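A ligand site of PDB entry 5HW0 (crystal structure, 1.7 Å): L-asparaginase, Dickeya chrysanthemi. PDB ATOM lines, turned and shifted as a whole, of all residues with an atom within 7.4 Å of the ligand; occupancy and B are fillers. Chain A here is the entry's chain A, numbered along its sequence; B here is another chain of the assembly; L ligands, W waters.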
ATOM      1  N   GLY A  14       9.746  -8.601 -31.166  1.00  0.00           N
ATOM      2  CA  GLY A  14      10.234  -7.247 -31.263  1.00  0.00           C
ATOM      3  C   GLY A  14      10.897  -6.833 -29.975  1.00  0.00           C
ATOM      4  O   GLY A  14      11.377  -7.668 -29.198  1.00  0.00           O
ATOM      5  N   GLY A  15      10.933  -5.531 -29.739  1.00  0.00           N
ATOM      6  CA  GLY A  15      11.548  -4.991 -28.556  1.00  0.00           C
ATOM      7  C   GLY A  15      13.015  -4.640 -28.754  1.00  0.00           C
ATOM      8  O   GLY A  15      13.701  -5.143 -29.641  1.00  0.00           O
ATOM      9  N   THR A  16      13.495  -3.746 -27.879  1.00  0.00           N
ATOM     10  CA  THR A  16      14.866  -3.257 -27.976  1.00  0.00           C
ATOM     11  C   THR A  16      15.907  -4.341 -27.692  1.00  0.00           C
ATOM     12  O   THR A  16      17.081  -4.153 -28.031  1.00  0.00           O
ATOM     13  CB  THR A  16      15.040  -2.072 -27.042  1.00  0.00           C
ATOM     14  OG1 THR A  16      15.706  -1.003 -27.727  1.00  0.00           O
ATOM     15  CG2 THR A  16      15.795  -2.470 -25.765  1.00  0.00           C
ATOM     16  N   ILE A  17      15.497  -5.458 -27.092  1.00  0.00           N
ATOM     17  CA  ILE A  17      16.439  -6.567 -26.905  1.00  0.00           C
ATOM     18  C   ILE A  17      16.994  -7.001 -28.250  1.00  0.00           C
ATOM     19  O   ILE A  17      18.127  -7.509 -28.329  1.00  0.00           O
ATOM     20  CB  ILE A  17      15.747  -7.720 -26.144  1.00  0.00           C
ATOM     21  CG1 ILE A  17      16.746  -8.815 -25.809  1.00  0.00           C
ATOM     22  CG2 ILE A  17      14.556  -8.275 -26.945  1.00  0.00           C
ATOM     23  CD1 ILE A  17      16.227  -9.832 -24.847  1.00  0.00           C
ATOM     24  N   ALA A  18      16.235  -6.765 -29.313  1.00  0.00           N
ATOM     25  CA  ALA A  18      16.696  -6.945 -30.692  1.00  0.00           C
ATOM     26  C   ALA A  18      17.106  -5.602 -31.280  1.00  0.00           C
ATOM     27  O   ALA A  18      16.282  -4.884 -31.868  1.00  0.00           O
ATOM     28  CB  ALA A  18      15.599  -7.585 -31.528  1.00  0.00           C
ATOM     29  N   GLY A  33      11.505  -3.248 -32.235  1.00  0.00           N
ATOM     30  CA  GLY A  33      12.767  -3.914 -32.515  1.00  0.00           C
ATOM     31  C   GLY A  33      13.262  -3.761 -33.936  1.00  0.00           C
ATOM     32  O   GLY A  33      12.468  -3.582 -34.871  1.00  0.00           O
ATOM     33  N   MET A  61       7.872  -5.686 -33.563  1.00  0.00           N
ATOM     34  CA  MET A  61       7.256  -4.413 -33.252  1.00  0.00           C
ATOM     35  C   MET A  61       7.664  -3.948 -31.865  1.00  0.00           C
ATOM     36  O   MET A  61       8.006  -4.751 -30.992  1.00  0.00           O
ATOM     37  CB  MET A  61       5.732  -4.493 -33.345  1.00  0.00           C
ATOM     38  CG  MET A  61       5.094  -5.336 -32.246  1.00  0.00           C
ATOM     39  SD  MET A  61       3.314  -5.385 -32.462  1.00  0.00           S
ATOM     40  CE  MET A  61       3.167  -6.655 -33.720  1.00  0.00           C
ATOM     41  N   ALA A  62       7.623  -2.643 -31.669  1.00  0.00           N
ATOM     42  CA  ALA A  62       7.712  -2.088 -30.321  1.00  0.00           C
ATOM     43  C   ALA A  62       6.473  -2.503 -29.533  1.00  0.00           C
ATOM     44  O   ALA A  62       5.355  -2.514 -30.055  1.00  0.00           O
ATOM     45  CB  ALA A  62       7.855  -0.571 -30.387  1.00  0.00           C
ATOM     46  N   SER A  63       6.667  -2.871 -28.263  1.00  0.00           N
ATOM     47  CA  SER A  63       5.576  -3.519 -27.546  1.00  0.00           C
ATOM     48  C   SER A  63       4.415  -2.587 -27.280  1.00  0.00           C
ATOM     49  O   SER A  63       3.297  -3.069 -27.026  1.00  0.00           O
ATOM     50  CB  SER A  63       6.077  -4.117 -26.219  1.00  0.00           C
ATOM     51  OG  SER A  63       6.306  -3.092 -25.259  1.00  0.00           O
ATOM     52  N   GLU A  64       4.618  -1.270 -27.332  1.00  0.00           N
ATOM     53  CA  GLU A  64       3.478  -0.367 -27.193  1.00  0.00           C
ATOM     54  C   GLU A  64       2.485  -0.510 -28.334  1.00  0.00           C
ATOM     55  O   GLU A  64       1.356  -0.009 -28.224  1.00  0.00           O
ATOM     56  CB  GLU A  64       3.940   1.091 -27.096  1.00  0.00           C
ATOM     57  CG  GLU A  64       4.678   1.648 -28.321  1.00  0.00           C
ATOM     58  CD  GLU A  64       6.186   1.504 -28.210  1.00  0.00           C
ATOM     59  OE1 GLU A  64       6.662   0.530 -27.594  1.00  0.00           O
ATOM     60  OE2 GLU A  64       6.908   2.380 -28.736  1.00  0.00           O
ATOM     61  N   ASN A  65       2.863  -1.192 -29.415  1.00  0.00           N
ATOM     62  CA  ASN A  65       1.963  -1.434 -30.528  1.00  0.00           C
ATOM     63  C   ASN A  65       1.442  -2.861 -30.570  1.00  0.00           C
ATOM     64  O   ASN A  65       0.668  -3.200 -31.474  1.00  0.00           O
ATOM     65  CB  ASN A  65       2.669  -1.078 -31.836  1.00  0.00           C
ATOM     66  CG  ASN A  65       2.650   0.414 -32.090  1.00  0.00           C
ATOM     67  OD1 ASN A  65       1.595   1.038 -32.033  1.00  0.00           O
ATOM     68  ND2 ASN A  65       3.824   1.000 -32.310  1.00  0.00           N
ATOM     69  N   HIS A  94      10.491  -9.764 -26.372  1.00  0.00           N
ATOM     70  CA  HIS A  94       9.357  -8.848 -26.331  1.00  0.00           C
ATOM     71  C   HIS A  94       9.875  -7.520 -25.806  1.00  0.00           C
ATOM     72  O   HIS A  94      10.878  -7.485 -25.091  1.00  0.00           O
ATOM     73  CB  HIS A  94       8.256  -9.437 -25.439  1.00  0.00           C
ATOM     74  CG  HIS A  94       6.882  -8.858 -25.628  1.00  0.00           C
ATOM     75  ND1 HIS A  94       6.510  -7.617 -25.134  1.00  0.00           N
ATOM     76  CD2 HIS A  94       5.751  -9.395 -26.151  1.00  0.00           C
ATOM     77  CE1 HIS A  94       5.237  -7.402 -25.399  1.00  0.00           C
ATOM     78  NE2 HIS A  94       4.751  -8.467 -26.006  1.00  0.00           N
ATOM     79  N   GLY A  95       9.211  -6.425 -26.170  1.00  0.00           N
ATOM     80  CA  GLY A  95       9.504  -5.145 -25.550  1.00  0.00           C
ATOM     81  C   GLY A  95       9.018  -5.120 -24.112  1.00  0.00           C
ATOM     82  O   GLY A  95       8.108  -5.848 -23.717  1.00  0.00           O
ATOM     83  N   THR A  96       9.661  -4.265 -23.296  1.00  0.00           N
ATOM     84  CA  THR A  96       9.346  -4.227 -21.867  1.00  0.00           C
ATOM     85  C   THR A  96       7.996  -3.578 -21.576  1.00  0.00           C
ATOM     86  O   THR A  96       7.352  -3.918 -20.578  1.00  0.00           O
ATOM     87  CB  THR A  96      10.420  -3.450 -21.089  1.00  0.00           C
ATOM     88  OG1 THR A  96      10.531  -2.111 -21.611  1.00  0.00           O
ATOM     89  CG2 THR A  96      11.771  -4.136 -21.178  1.00  0.00           C
ATOM     90  N   ASP A  97       7.541  -2.651 -22.424  1.00  0.00           N
ATOM     91  CA  ASP A  97       6.458  -1.762 -22.012  1.00  0.00           C
ATOM     92  C   ASP A  97       5.151  -2.500 -21.777  1.00  0.00           C
ATOM     93  O   ASP A  97       4.414  -2.174 -20.838  1.00  0.00           O
ATOM     94  CB  ASP A  97       6.274  -0.649 -23.039  1.00  0.00           C
ATOM     95  CG  ASP A  97       7.411   0.336 -23.014  1.00  0.00           C
ATOM     96  OD1 ASP A  97       8.246   0.261 -22.089  1.00  0.00           O
ATOM     97  OD2 ASP A  97       7.487   1.186 -23.921  1.00  0.00           O
ATOM     98  N   THR A  98       4.820  -3.498 -22.605  1.00  0.00           N
ATOM     99  CA  THR A  98       3.583  -4.244 -22.403  1.00  0.00           C
ATOM    100  C   THR A  98       3.816  -5.748 -22.263  1.00  0.00           C
ATOM    101  O   THR A  98       2.874  -6.535 -22.386  1.00  0.00           O
ATOM    102  CB  THR A  98       2.558  -3.993 -23.525  1.00  0.00           C
ATOM    103  OG1 THR A  98       2.992  -4.581 -24.753  1.00  0.00           O
ATOM    104  CG2 THR A  98       2.333  -2.508 -23.711  1.00  0.00           C
ATOM    105  N   VAL A  99       5.040  -6.167 -21.961  1.00  0.00           N
ATOM    106  CA  VAL A  99       5.295  -7.605 -21.790  1.00  0.00           C
ATOM    107  C   VAL A  99       4.388  -8.186 -20.715  1.00  0.00           C
ATOM    108  O   VAL A  99       3.974  -9.348 -20.808  1.00  0.00           O
ATOM    109  CB  VAL A  99       6.789  -7.871 -21.475  1.00  0.00           C
ATOM    110  CG1 VAL A  99       7.149  -7.399 -20.050  1.00  0.00           C
ATOM    111  CG2 VAL A  99       7.111  -9.344 -21.644  1.00  0.00           C
ATOM    112  N   ALA A 120      13.077  -9.645 -22.049  1.00  0.00           N
ATOM    113  CA  ALA A 120      13.111  -8.291 -22.592  1.00  0.00           C
ATOM    114  C   ALA A 120      14.394  -7.619 -22.109  1.00  0.00           C
ATOM    115  O   ALA A 120      15.163  -8.196 -21.335  1.00  0.00           O
ATOM    116  CB  ALA A 120      11.865  -7.506 -22.155  1.00  0.00           C
ATOM    117  N   ALA A 121      14.628  -6.402 -22.577  1.00  0.00           N
ATOM    118  CA  ALA A 121      15.805  -5.644 -22.161  1.00  0.00           C
ATOM    119  C   ALA A 121      15.432  -4.175 -21.995  1.00  0.00           C
ATOM    120  O   ALA A 121      14.700  -3.610 -22.819  1.00  0.00           O
ATOM    121  CB  ALA A 121      16.942  -5.754 -23.187  1.00  0.00           C
ATOM    122  N   MET A 122      15.952  -3.550 -20.953  1.00  0.00           N
ATOM    123  CA  MET A 122      15.725  -2.129 -20.754  1.00  0.00           C
ATOM    124  C   MET A 122      16.706  -1.244 -21.498  1.00  0.00           C
ATOM    125  O   MET A 122      16.400  -0.082 -21.767  1.00  0.00           O
ATOM    126  CB  MET A 122      15.733  -1.808 -19.262  1.00  0.00           C
ATOM    127  CG  MET A 122      14.478  -2.287 -18.530  1.00  0.00           C
ATOM    128  SD  MET A 122      12.991  -1.425 -19.118  1.00  0.00           S
ATOM    129  CE  MET A 122      13.215   0.187 -18.364  1.00  0.00           C
ATOM    130  N   ARG A 123      17.870  -1.775 -21.867  1.00  0.00           N
ATOM    131  CA  ARG A 123      18.780  -1.014 -22.712  1.00  0.00           C
ATOM    132  C   ARG A 123      18.831  -1.633 -24.104  1.00  0.00           C
ATOM    133  O   ARG A 123      18.751  -2.850 -24.235  1.00  0.00           O
ATOM    134  CB  ARG A 123      20.191  -0.988 -22.119  1.00  0.00           C
ATOM    135  CG  ARG A 123      20.308  -0.186 -20.826  1.00  0.00           C
ATOM    136  CD  ARG A 123      21.653  -0.405 -20.146  1.00  0.00           C
ATOM    137  NE  ARG A 123      21.758   0.363 -18.917  1.00  0.00           N
ATOM    138  CZ  ARG A 123      22.657   0.129 -17.967  1.00  0.00           C
ATOM    139  NH1 ARG A 123      23.529  -0.869 -18.099  1.00  0.00           N
ATOM    140  NH2 ARG A 123      22.676   0.887 -16.875  1.00  0.00           N
ATOM    141  N   PRO A 124      18.958  -0.813 -25.146  1.00  0.00           N
ATOM    142  CA  PRO A 124      19.065  -1.378 -26.498  1.00  0.00           C
ATOM    143  C   PRO A 124      20.335  -2.208 -26.637  1.00  0.00           C
ATOM    144  O   PRO A 124      21.336  -1.974 -25.962  1.00  0.00           O
ATOM    145  CB  PRO A 124      19.106  -0.133 -27.408  1.00  0.00           C
ATOM    146  CG  PRO A 124      19.545   0.980 -26.517  1.00  0.00           C
ATOM    147  CD  PRO A 124      18.986   0.650 -25.145  1.00  0.00           C
ATOM    148  N   LYS A 169       6.009  -3.865 -14.687  1.00  0.00           N
ATOM    149  CA  LYS A 169       7.031  -2.844 -14.883  1.00  0.00           C
ATOM    150  C   LYS A 169       6.732  -1.692 -13.930  1.00  0.00           C
ATOM    151  O   LYS A 169       5.751  -0.973 -14.118  1.00  0.00           O
ATOM    152  CB  LYS A 169       7.040  -2.375 -16.343  1.00  0.00           C
ATOM    153  CG  LYS A 169       8.219  -1.474 -16.702  1.00  0.00           C
ATOM    154  CD  LYS A 169       8.305  -1.174 -18.215  1.00  0.00           C
ATOM    155  CE  LYS A 169       9.507  -0.241 -18.503  1.00  0.00           C
ATOM    156  NZ  LYS A 169       9.761  -0.147 -19.973  1.00  0.00           N
ATOM    157  N   PHE A 178      11.290  -4.596 -13.221  1.00  0.00           N
ATOM    158  CA  PHE A 178      10.280  -5.648 -13.068  1.00  0.00           C
ATOM    159  C   PHE A 178      10.323  -6.204 -11.647  1.00  0.00           C
ATOM    160  O   PHE A 178      11.321  -6.818 -11.239  1.00  0.00           O
ATOM    161  CB  PHE A 178      10.469  -6.725 -14.130  1.00  0.00           C
ATOM    162  CG  PHE A 178       9.990  -6.262 -15.481  1.00  0.00           C
ATOM    163  CD1 PHE A 178       8.635  -6.295 -15.797  1.00  0.00           C
ATOM    164  CD2 PHE A 178      10.884  -5.736 -16.408  1.00  0.00           C
ATOM    165  CE1 PHE A 178       8.171  -5.838 -17.036  1.00  0.00           C
ATOM    166  CE2 PHE A 178      10.449  -5.273 -17.651  1.00  0.00           C
ATOM    167  CZ  PHE A 178       9.076  -5.317 -17.970  1.00  0.00           C
ATOM    168  N   MET B 251       2.545   3.652 -21.227  1.00  0.00           N
ATOM    169  CA  MET B 251       3.295   2.415 -21.138  1.00  0.00           C
ATOM    170  C   MET B 251       4.792   2.719 -20.995  1.00  0.00           C
ATOM    171  O   MET B 251       5.334   3.558 -21.711  1.00  0.00           O
ATOM    172  CB  MET B 251       3.047   1.573 -22.389  1.00  0.00           C
ATOM    173  CG  MET B 251       1.549   1.309 -22.639  1.00  0.00           C
ATOM    174  SD  MET B 251       1.134   0.623 -24.267  1.00  0.00           S
ATOM    175  CE  MET B 251       0.785   2.106 -25.223  1.00  0.00           C
ATOM    176  N   GLY B 252       5.448   2.031 -20.058  1.00  0.00           N
ATOM    177  CA  GLY B 252       6.868   2.243 -19.855  1.00  0.00           C
ATOM    178  C   GLY B 252       7.200   3.719 -19.695  1.00  0.00           C
ATOM    179  O   GLY B 252       6.516   4.473 -18.994  1.00  0.00           O
ATOM    180  N   ALA B 253       8.238   4.161 -20.410  1.00  0.00           N
ATOM    181  CA  ALA B 253       8.689   5.550 -20.337  1.00  0.00           C
ATOM    182  C   ALA B 253       7.880   6.439 -21.289  1.00  0.00           C
ATOM    183  O   ALA B 253       8.412   7.032 -22.224  1.00  0.00           O
ATOM    184  CB  ALA B 253      10.188   5.621 -20.630  1.00  0.00           C
ATOM    185  N   GLY B 254       6.578   6.501 -21.025  1.00  0.00           N
ATOM    186  CA  GLY B 254       5.703   7.344 -21.835  1.00  0.00           C
ATOM    187  C   GLY B 254       5.627   6.921 -23.287  1.00  0.00           C
ATOM    188  O   GLY B 254       5.418   7.777 -24.161  1.00  0.00           O
ATOM    189  N   SER B 255       5.787   5.636 -23.570  1.00  0.00           N
ATOM    190  CA  SER B 255       5.681   5.152 -24.943  1.00  0.00           C
ATOM    191  C   SER B 255       4.243   5.227 -25.437  1.00  0.00           C
ATOM    192  O   SER B 255       3.287   5.075 -24.682  1.00  0.00           O
ATOM    193  CB  SER B 255       6.151   3.696 -25.054  1.00  0.00           C
ATOM    194  OG  SER B 255       7.502   3.581 -24.668  1.00  0.00           O
ATOM    195  N   VAL B 256       4.093   5.445 -26.743  1.00  0.00           N
ATOM    196  CA  VAL B 256       2.813   5.740 -27.360  1.00  0.00           C
ATOM    197  C   VAL B 256       2.602   4.804 -28.544  1.00  0.00           C
ATOM    198  O   VAL B 256       3.505   4.647 -29.379  1.00  0.00           O
ATOM    199  CB  VAL B 256       2.724   7.211 -27.809  1.00  0.00           C
ATOM    200  CG1 VAL B 256       1.283   7.580 -28.031  1.00  0.00           C
ATOM    201  CG2 VAL B 256       3.368   8.142 -26.787  1.00  0.00           C
HETATM  202  N1  LIG L   1       8.858   1.111 -26.083  1.00  0.00           N
HETATM  203  C1  LIG L   1       9.807   0.038 -26.369  1.00  0.00           C
HETATM  204  C2  LIG L   1       9.133  -1.342 -26.325  1.00  0.00           C
HETATM  205  O1  LIG L   1       9.339  -2.174 -27.206  1.00  0.00           O
HETATM  206  C3  LIG L   1      10.965   0.081 -25.381  1.00  0.00           C
HETATM  207  C4  LIG L   1      12.097  -0.893 -25.699  1.00  0.00           C
HETATM  208  C5  LIG L   1      11.935  -2.239 -25.017  1.00  0.00           C
HETATM  209  O2  LIG L   1      12.303  -3.263 -25.621  1.00  0.00           O
HETATM  210  O3  LIG L   1      11.426  -2.283 -23.882  1.00  0.00           O
HETATM  211  O4  LIG L   1       8.396  -1.659 -25.386  1.00  0.00           O
HETATM  212  O   HOH W   1      11.023  -1.696 -29.292  1.00  0.00           O
HETATM  213  O   HOH W   2      13.038  -5.672 -25.055  1.00  0.00           O
HETATM  214  O   HOH W   3      10.069   3.461 -25.666  1.00  0.00           O
HETATM  215  O   HOH W   4       9.462   2.719 -28.616  1.00  0.00           O
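The side-chain hydroxyl of Thr 96 is in hydrogen-bond range of an oxygen (O3) of the ligand (2.4 Å).
An oxygen (O3) of the ligand sits at hydrogen-bond distance from the backbone NH (N) of Thr 96 (2.7 Å).
A nitrogen (N1) of the ligand lies within salt-bridge range of the side-chain carboxylate of Asp 97, 2.6 Å away.
The side-chain hydroxyl (OG) of Ser 63 sits at hydrogen-bond distance from an oxygen (O4) of the ligand, at 2.5 Å.
O4 of the ligand lies within hydrogen-bond range of N of Asp 97 (3.2 Å).
N of Thr 16 lies within hydrogen-bond range of O2 of the ligand, 2.6 Å away.
The backbone NH of Ser 63 lies within hydrogen-bond range of an oxygen (O1) of the ligand (3.0 Å).
The side-chain carboxylate (OE1) of Glu 64 lies within salt-bridge range of a nitrogen (N1) of the ligand (2.7 Å).
N1 of the ligand is in hydrogen-bond range of OG of Ser 255 of chain B, at 3.2 Å.
Merely in contact with the ligand: Gly 95, Gly 15, Ala 62 and Ala 121.
Ten residues have an atom within 4 Å of the ligand: Gly 15, Thr 16, Ala 62, Ser 63, Glu 64, Gly 95, Thr 96, Asp 97, Ala 121 and Ser 255 of chain B.
The nearest printed residue that does not touch the ligand is Ile 17 (4.1 Å).
N of Gly 15 sits at hydrogen-bond distance from O of Met 61, 3.3 Å away.
OD1 of Asp 97 lies within hydrogen-bond range of OG1 of Thr 96, at 3.3 Å.
O of Ser 63 is in hydrogen-bond range of OG1 of Thr 98 (2.7 Å).
OG1 of Thr 96 is in hydrogen-bond range of NZ of Lys 169, at 2.7 Å.
OG1 of Thr 96 sits at hydrogen-bond distance from SD of Met 122 (3.6 Å).
The side-chain hydroxyl (OG) of Ser 255 of chain B sits at hydrogen-bond distance from the side-chain carboxylate (OD2) of Asp 97, 2.5 Å away.
The side-chain carboxylate of Asp 97 lies within salt-bridge range of the side-chain amino group of Lys 169 (2.6 Å).
The side-chain hydroxyl (OG) of Ser 63 sits at hydrogen-bond distance from the backbone NH (N) of Asp 97 (3.1 Å).
Water W3 lies within hydrogen-bond range of a nitrogen (N1) of the ligand (2.7 Å) and the side-chain hydroxyl (OG) of Ser 255 of chain B (2.8 Å).
Water W1 lies within hydrogen-bond range of O1 of the ligand (2.7 Å) and N of Gly 33 (3.4 Å).
Water W4 lies within hydrogen-bond range of the side-chain carboxylate of Glu 64 (2.6 Å) and a nitrogen (N1) of the ligand (3.1 Å).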
